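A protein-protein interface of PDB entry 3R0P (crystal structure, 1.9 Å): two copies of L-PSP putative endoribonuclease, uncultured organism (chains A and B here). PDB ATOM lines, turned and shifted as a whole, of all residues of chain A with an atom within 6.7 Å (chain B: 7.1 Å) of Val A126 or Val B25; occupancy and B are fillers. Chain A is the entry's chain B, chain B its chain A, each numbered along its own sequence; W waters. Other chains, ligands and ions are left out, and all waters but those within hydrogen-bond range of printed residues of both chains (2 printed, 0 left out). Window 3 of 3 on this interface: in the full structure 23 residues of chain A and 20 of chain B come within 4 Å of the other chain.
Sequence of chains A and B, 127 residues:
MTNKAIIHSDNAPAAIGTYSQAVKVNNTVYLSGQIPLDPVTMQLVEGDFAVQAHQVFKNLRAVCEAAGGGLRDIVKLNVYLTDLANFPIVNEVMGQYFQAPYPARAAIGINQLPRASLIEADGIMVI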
ATOM      1  N   ASN A  27     -10.133  14.855  -9.577  1.00  0.00           N
ATOM      2  CA  ASN A  27     -10.545  13.735  -8.735  1.00  0.00           C
ATOM      3  C   ASN A  27      -9.450  12.708  -8.465  1.00  0.00           C
ATOM      4  O   ASN A  27      -9.681  11.710  -7.778  1.00  0.00           O
ATOM      5  CB  ASN A  27     -11.786  13.056  -9.317  1.00  0.00           C
ATOM      6  CG  ASN A  27     -13.008  13.949  -9.255  1.00  0.00           C
ATOM      7  OD1 ASN A  27     -13.746  14.086 -10.233  1.00  0.00           O
ATOM      8  ND2 ASN A  27     -13.217  14.584  -8.102  1.00  0.00           N
ATOM      9  N   THR A  28      -8.257  12.949  -8.997  1.00  0.00           N
ATOM     10  CA  THR A  28      -7.168  12.006  -8.802  1.00  0.00           C
ATOM     11  C   THR A  28      -6.251  12.489  -7.687  1.00  0.00           C
ATOM     12  O   THR A  28      -5.920  13.669  -7.619  1.00  0.00           O
ATOM     13  CB  THR A  28      -6.385  11.775 -10.106  1.00  0.00           C
ATOM     14  OG1 THR A  28      -7.275  11.256 -11.100  1.00  0.00           O
ATOM     15  CG2 THR A  28      -5.281  10.768  -9.889  1.00  0.00           C
ATOM     16  N   VAL A  29      -5.854  11.583  -6.800  1.00  0.00           N
ATOM     17  CA  VAL A  29      -4.997  11.952  -5.671  1.00  0.00           C
ATOM     18  C   VAL A  29      -3.712  11.135  -5.682  1.00  0.00           C
ATOM     19  O   VAL A  29      -3.745   9.900  -5.696  1.00  0.00           O
ATOM     20  CB  VAL A  29      -5.730  11.730  -4.325  1.00  0.00           C
ATOM     21  CG1 VAL A  29      -4.869  12.197  -3.161  1.00  0.00           C
ATOM     22  CG2 VAL A  29      -7.059  12.464  -4.336  1.00  0.00           C
ATOM     23  N   ARG A  72     -10.981   2.963   0.127  1.00  0.00           N
ATOM     24  CA  ARG A  72     -11.725   2.330  -0.956  1.00  0.00           C
ATOM     25  C   ARG A  72     -11.525   3.051  -2.294  1.00  0.00           C
ATOM     26  O   ARG A  72     -11.790   2.487  -3.351  1.00  0.00           O
ATOM     27  CB  ARG A  72     -13.215   2.244  -0.628  1.00  0.00           C
ATOM     28  CG  ARG A  72     -13.962   3.545  -0.843  1.00  0.00           C
ATOM     29  CD  ARG A  72     -15.443   3.381  -0.522  1.00  0.00           C
ATOM     30  NE  ARG A  72     -16.216   4.549  -0.932  1.00  0.00           N
ATOM     31  CZ  ARG A  72     -17.073   4.559  -1.948  1.00  0.00           C
ATOM     32  NH1 ARG A  72     -17.280   3.452  -2.655  1.00  0.00           N
ATOM     33  NH2 ARG A  72     -17.730   5.673  -2.248  1.00  0.00           N
ATOM     34  N   ASP A  73     -11.048   4.294  -2.255  1.00  0.00           N
ATOM     35  CA  ASP A  73     -10.847   5.043  -3.493  1.00  0.00           C
ATOM     36  C   ASP A  73      -9.452   4.841  -4.099  1.00  0.00           C
ATOM     37  O   ASP A  73      -9.145   5.373  -5.166  1.00  0.00           O
ATOM     38  CB  ASP A  73     -11.100   6.533  -3.255  1.00  0.00           C
ATOM     39  CG  ASP A  73     -12.515   6.810  -2.784  1.00  0.00           C
ATOM     40  OD1 ASP A  73     -13.468   6.375  -3.473  1.00  0.00           O
ATOM     41  OD2 ASP A  73     -12.668   7.448  -1.716  1.00  0.00           O
ATOM     42  N   ILE A  74      -8.604   4.086  -3.415  1.00  0.00           N
ATOM     43  CA  ILE A  74      -7.273   3.807  -3.945  1.00  0.00           C
ATOM     44  C   ILE A  74      -7.415   2.887  -5.151  1.00  0.00           C
ATOM     45  O   ILE A  74      -8.105   1.859  -5.086  1.00  0.00           O
ATOM     46  CB  ILE A  74      -6.370   3.186  -2.866  1.00  0.00           C
ATOM     47  CG1 ILE A  74      -6.037   4.253  -1.807  1.00  0.00           C
ATOM     48  CG2 ILE A  74      -5.098   2.621  -3.479  1.00  0.00           C
ATOM     49  CD1 ILE A  74      -5.122   3.784  -0.708  1.00  0.00           C
ATOM     50  N   VAL A  75      -6.798   3.271  -6.266  1.00  0.00           N
ATOM     51  CA  VAL A  75      -6.858   2.466  -7.488  1.00  0.00           C
ATOM     52  C   VAL A  75      -5.572   1.672  -7.721  1.00  0.00           C
ATOM     53  O   VAL A  75      -5.576   0.632  -8.381  1.00  0.00           O
ATOM     54  CB  VAL A  75      -7.144   3.339  -8.736  1.00  0.00           C
ATOM     55  CG1 VAL A  75      -8.553   3.939  -8.656  1.00  0.00           C
ATOM     56  CG2 VAL A  75      -6.066   4.440  -8.912  1.00  0.00           C
ATOM     57  N   ILE A 124      -2.153   5.744  -5.684  1.00  0.00           N
ATOM     58  CA  ILE A 124      -2.989   6.674  -6.401  1.00  0.00           C
ATOM     59  C   ILE A 124      -4.432   6.390  -6.038  1.00  0.00           C
ATOM     60  O   ILE A 124      -4.863   5.237  -5.941  1.00  0.00           O
ATOM     61  CB  ILE A 124      -2.783   6.563  -7.932  1.00  0.00           C
ATOM     62  CG1 ILE A 124      -1.338   6.946  -8.294  1.00  0.00           C
ATOM     63  CG2 ILE A 124      -3.766   7.459  -8.653  1.00  0.00           C
ATOM     64  CD1 ILE A 124      -1.000   6.768  -9.766  1.00  0.00           C
ATOM     65  N   MET A 125      -5.177   7.463  -5.833  1.00  0.00           N
ATOM     66  CA  MET A 125      -6.565   7.379  -5.467  1.00  0.00           C
ATOM     67  C   MET A 125      -7.364   8.158  -6.509  1.00  0.00           C
ATOM     68  O   MET A 125      -6.905   9.188  -7.005  1.00  0.00           O
ATOM     69  CB  MET A 125      -6.688   7.971  -4.045  1.00  0.00           C
ATOM     70  CG  MET A 125      -8.018   8.471  -3.586  1.00  0.00           C
ATOM     71  SD  MET A 125      -7.821   9.289  -1.955  1.00  0.00           S
ATOM     72  CE  MET A 125      -9.497   9.850  -1.766  1.00  0.00           C
ATOM     73  N   VAL A 126      -8.530   7.647  -6.880  1.00  0.00           N
ATOM     74  CA  VAL A 126      -9.458   8.387  -7.721  1.00  0.00           C
ATOM     75  C   VAL A 126     -10.829   8.371  -7.064  1.00  0.00           C
ATOM     76  O   VAL A 126     -11.382   7.299  -6.794  1.00  0.00           O
ATOM     77  CB  VAL A 126      -9.577   7.781  -9.133  1.00  0.00           C
ATOM     78  CG1 VAL A 126     -10.515   8.620  -9.989  1.00  0.00           C
ATOM     79  CG2 VAL A 126      -8.211   7.668  -9.792  1.00  0.00           C
ATOM     80  N   ILE A 127     -11.379   9.551  -6.803  1.00  0.00           N
ATOM     81  CA  ILE A 127     -12.658   9.645  -6.104  1.00  0.00           C
ATOM     82  C   ILE A 127     -13.864   9.595  -7.043  1.00  0.00           C
ATOM     83  O   ILE A 127     -13.791  10.030  -8.192  1.00  0.00           O
ATOM     84  CB  ILE A 127     -12.726  10.908  -5.237  1.00  0.00           C
ATOM     85  CG1 ILE A 127     -11.472  11.008  -4.371  1.00  0.00           C
ATOM     86  CG2 ILE A 127     -13.988  10.891  -4.372  1.00  0.00           C
ATOM     87  CD1 ILE A 127     -11.365  12.304  -3.603  1.00  0.00           C
ATOM     88  N   ASN B   3     -18.216   3.795 -11.512  1.00  0.00           N
ATOM     89  CA  ASN B   3     -17.005   4.593 -11.357  1.00  0.00           C
ATOM     90  C   ASN B   3     -15.743   3.769 -11.606  1.00  0.00           C
ATOM     91  O   ASN B   3     -14.994   4.043 -12.537  1.00  0.00           O
ATOM     92  CB  ASN B   3     -16.964   5.245  -9.973  1.00  0.00           C
ATOM     93  CG  ASN B   3     -15.789   6.191  -9.804  1.00  0.00           C
ATOM     94  OD1 ASN B   3     -14.810   5.864  -9.136  1.00  0.00           O
ATOM     95  ND2 ASN B   3     -15.883   7.373 -10.405  1.00  0.00           N
ATOM     96  N   LYS B   4     -15.506   2.761 -10.775  1.00  0.00           N
ATOM     97  CA  LYS B   4     -14.355   1.891 -10.973  1.00  0.00           C
ATOM     98  C   LYS B   4     -14.810   0.573 -11.593  1.00  0.00           C
ATOM     99  O   LYS B   4     -15.853   0.029 -11.227  1.00  0.00           O
ATOM    100  CB  LYS B   4     -13.633   1.601  -9.652  1.00  0.00           C
ATOM    101  CG  LYS B   4     -13.543   2.768  -8.679  1.00  0.00           C
ATOM    102  CD  LYS B   4     -12.448   3.746  -9.041  1.00  0.00           C
ATOM    103  CE  LYS B   4     -12.137   4.647  -7.855  1.00  0.00           C
ATOM    104  NZ  LYS B   4     -11.757   3.838  -6.664  1.00  0.00           N
ATOM    105  N   ALA B   5     -14.030   0.066 -12.537  1.00  0.00           N
ATOM    106  CA  ALA B   5     -14.278  -1.260 -13.072  1.00  0.00           C
ATOM    107  C   ALA B   5     -13.069  -2.122 -12.784  1.00  0.00           C
ATOM    108  O   ALA B   5     -11.922  -1.694 -12.976  1.00  0.00           O
ATOM    109  CB  ALA B   5     -14.551  -1.203 -14.565  1.00  0.00           C
ATOM    110  N   VAL B  23      -7.408  -1.885 -12.420  1.00  0.00           N
ATOM    111  CA  VAL B  23      -8.591  -1.095 -12.108  1.00  0.00           C
ATOM    112  C   VAL B  23      -8.701  -0.024 -13.170  1.00  0.00           C
ATOM    113  O   VAL B  23      -7.734   0.686 -13.446  1.00  0.00           O
ATOM    114  CB  VAL B  23      -8.472  -0.394 -10.738  1.00  0.00           C
ATOM    115  CG1 VAL B  23      -9.648   0.542 -10.509  1.00  0.00           C
ATOM    116  CG2 VAL B  23      -8.374  -1.420  -9.623  1.00  0.00           C
ATOM    117  N   LYS B  24      -9.884   0.113 -13.748  1.00  0.00           N
ATOM    118  CA  LYS B  24     -10.097   1.092 -14.808  1.00  0.00           C
ATOM    119  C   LYS B  24     -11.088   2.153 -14.357  1.00  0.00           C
ATOM    120  O   LYS B  24     -12.162   1.829 -13.857  1.00  0.00           O
ATOM    121  CB  LYS B  24     -10.619   0.386 -16.062  1.00  0.00           C
ATOM    122  CG  LYS B  24     -10.986   1.303 -17.201  1.00  0.00           C
ATOM    123  CD  LYS B  24     -11.394   0.466 -18.407  1.00  0.00           C
ATOM    124  CE  LYS B  24     -11.844   1.324 -19.575  1.00  0.00           C
ATOM    125  NZ  LYS B  24     -12.327   0.461 -20.698  1.00  0.00           N
ATOM    126  N   VAL B  25     -10.724   3.419 -14.539  1.00  0.00           N
ATOM    127  CA  VAL B  25     -11.579   4.528 -14.143  1.00  0.00           C
ATOM    128  C   VAL B  25     -11.447   5.659 -15.165  1.00  0.00           C
ATOM    129  O   VAL B  25     -10.356   6.188 -15.374  1.00  0.00           O
ATOM    130  CB  VAL B  25     -11.247   5.016 -12.708  1.00  0.00           C
ATOM    131  CG1 VAL B  25      -9.755   5.008 -12.467  1.00  0.00           C
ATOM    132  CG2 VAL B  25     -11.841   6.398 -12.447  1.00  0.00           C
ATOM    133  N   ASN B  26     -12.552   5.988 -15.834  1.00  0.00           N
ATOM    134  CA  ASN B  26     -12.564   7.050 -16.843  1.00  0.00           C
ATOM    135  C   ASN B  26     -11.433   6.948 -17.884  1.00  0.00           C
ATOM    136  O   ASN B  26     -10.703   7.913 -18.114  1.00  0.00           O
ATOM    137  CB  ASN B  26     -12.535   8.431 -16.170  1.00  0.00           C
ATOM    138  CG  ASN B  26     -12.920   9.562 -17.124  1.00  0.00           C
ATOM    139  OD1 ASN B  26     -13.830   9.415 -17.946  1.00  0.00           O
ATOM    140  ND2 ASN B  26     -12.221  10.697 -17.019  1.00  0.00           N
ATOM    141  N   ASN B  27     -11.292   5.785 -18.513  1.00  0.00           N
ATOM    142  CA  ASN B  27     -10.299   5.610 -19.587  1.00  0.00           C
ATOM    143  C   ASN B  27      -8.827   5.491 -19.150  1.00  0.00           C
ATOM    144  O   ASN B  27      -7.943   5.276 -19.987  1.00  0.00           O
ATOM    145  CB  ASN B  27     -10.435   6.704 -20.654  1.00  0.00           C
ATOM    146  CG  ASN B  27     -11.692   6.557 -21.494  1.00  0.00           C
ATOM    147  OD1 ASN B  27     -12.197   5.449 -21.705  1.00  0.00           O
ATOM    148  ND2 ASN B  27     -12.202   7.681 -21.986  1.00  0.00           N
ATOM    149  N   THR B  28      -8.554   5.643 -17.859  1.00  0.00           N
ATOM    150  CA  THR B  28      -7.229   5.326 -17.341  1.00  0.00           C
ATOM    151  C   THR B  28      -7.236   3.965 -16.657  1.00  0.00           C
ATOM    152  O   THR B  28      -8.117   3.672 -15.838  1.00  0.00           O
ATOM    153  CB  THR B  28      -6.717   6.414 -16.376  1.00  0.00           C
ATOM    154  OG1 THR B  28      -6.680   7.664 -17.066  1.00  0.00           O
ATOM    155  CG2 THR B  28      -5.319   6.087 -15.876  1.00  0.00           C
ATOM    156  N   VAL B  29      -6.267   3.124 -16.995  1.00  0.00           N
ATOM    157  CA  VAL B  29      -6.193   1.788 -16.406  1.00  0.00           C
ATOM    158  C   VAL B  29      -4.912   1.629 -15.606  1.00  0.00           C
ATOM    159  O   VAL B  29      -3.808   1.780 -16.138  1.00  0.00           O
ATOM    160  CB  VAL B  29      -6.250   0.694 -17.484  1.00  0.00           C
ATOM    161  CG1 VAL B  29      -6.179  -0.712 -16.860  1.00  0.00           C
ATOM    162  CG2 VAL B  29      -7.505   0.853 -18.281  1.00  0.00           C
ATOM    163  N   TYR B  30      -5.072   1.341 -14.320  1.00  0.00           N
ATOM    164  CA  TYR B  30      -3.948   1.073 -13.434  1.00  0.00           C
ATOM    165  C   TYR B  30      -3.637  -0.418 -13.378  1.00  0.00           C
ATOM    166  O   TYR B  30      -4.439  -1.212 -12.877  1.00  0.00           O
ATOM    167  CB  TYR B  30      -4.249   1.632 -12.039  1.00  0.00           C
ATOM    168  CG  TYR B  30      -4.394   3.135 -12.104  1.00  0.00           C
ATOM    169  CD1 TYR B  30      -3.297   3.953 -11.900  1.00  0.00           C
ATOM    170  CD2 TYR B  30      -5.601   3.731 -12.460  1.00  0.00           C
ATOM    171  CE1 TYR B  30      -3.398   5.315 -11.988  1.00  0.00           C
ATOM    172  CE2 TYR B  30      -5.701   5.131 -12.552  1.00  0.00           C
ATOM    173  CZ  TYR B  30      -4.598   5.900 -12.313  1.00  0.00           C
ATOM    174  OH  TYR B  30      -4.665   7.282 -12.398  1.00  0.00           O
HETATM  175  O   HOH W   1     -14.169   4.424  -5.302  1.00  0.00           O
HETATM  176  O   HOH W   2      -6.625   8.953 -12.966  1.00  0.00           O
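Among the printed residues, pairs that only touch across the chains: Val A126 with Val B25 (3.6 Å), Ile A124 with Tyr B30 (3.6 Å), Arg A72 with Lys B4 (3.6 Å), Val A75 with Tyr B30 (3.6 Å), Val A75 with Val B23 (3.7 Å) and Val A75 with Lys B4 (3.7 Å).
Water W2 lies within hydrogen-bond range of the side-chain hydroxyl (OH) of Tyr B30 (2.6 Å) and the side-chain hydroxyl (OG1) of Thr A28 (3.0 Å). Water W1 bridges OD1 of Asp A73 and NZ of Lys B4.
The side-chain amino group of Lys B4 is in hydrogen-bond range of the backbone carbonyl oxygen of Asp A73 (3.4 Å). The side-chain amino group (NZ) of Lys B4 sits close to the backbone carbonyl oxygen (O) of Val A126, at 3.5 Å.
Printed residues of chain B within 4 Å of Val A75: Lys B4, Val B23 and Tyr B30. Printed residues of chain B within 4 Å of Ile A124: Tyr B30 (3.6 Å). Of the printed residues of chain B, Val A126 touches Lys B4 and Val B25. Printed residues of chain A within 4 Å of Lys B4: Arg A72 (3.6 Å), Asp A73 (3.4 Å), Val A75 (3.7 Å) and Val A126 (3.0 Å). Val B25 touches just one residue of chain A: Val A126 (3.6 Å). Thr B28 touches none of the printed residues of chain A. The nearest printed residue of chain B that does not touch Val A126 is Asn B3 (4.4 Å).
The backbone NH (N) of Tyr B30 sits at hydrogen-bond distance from the backbone carbonyl oxygen (O) of Val B23 (2.9 Å). The backbone NH of Val A75 lies within hydrogen-bond range of the backbone carbonyl oxygen of Ile A124 (2.8 Å). O of Asp A73 is in hydrogen-bond range of N of Val A126, at 2.9 Å.
Of the 11 printed residues of chain A, 5 touch a printed residue of chain B. Hydrophobic or aromatic side chains of chain A that line the printed part of chain B: Val A75, Ile A124 and Val A126. Hydrophobic or aromatic side chains of chain B that line the printed part of chain A: Val B23, Val B25 and Tyr B30. Among the printed residues, 8 pairs touch across the chains.
3 positions are printed for both chains. Of the 8 pairs that touch across the chains among the printed residues, none has its exchanged pair printed and touching as well.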
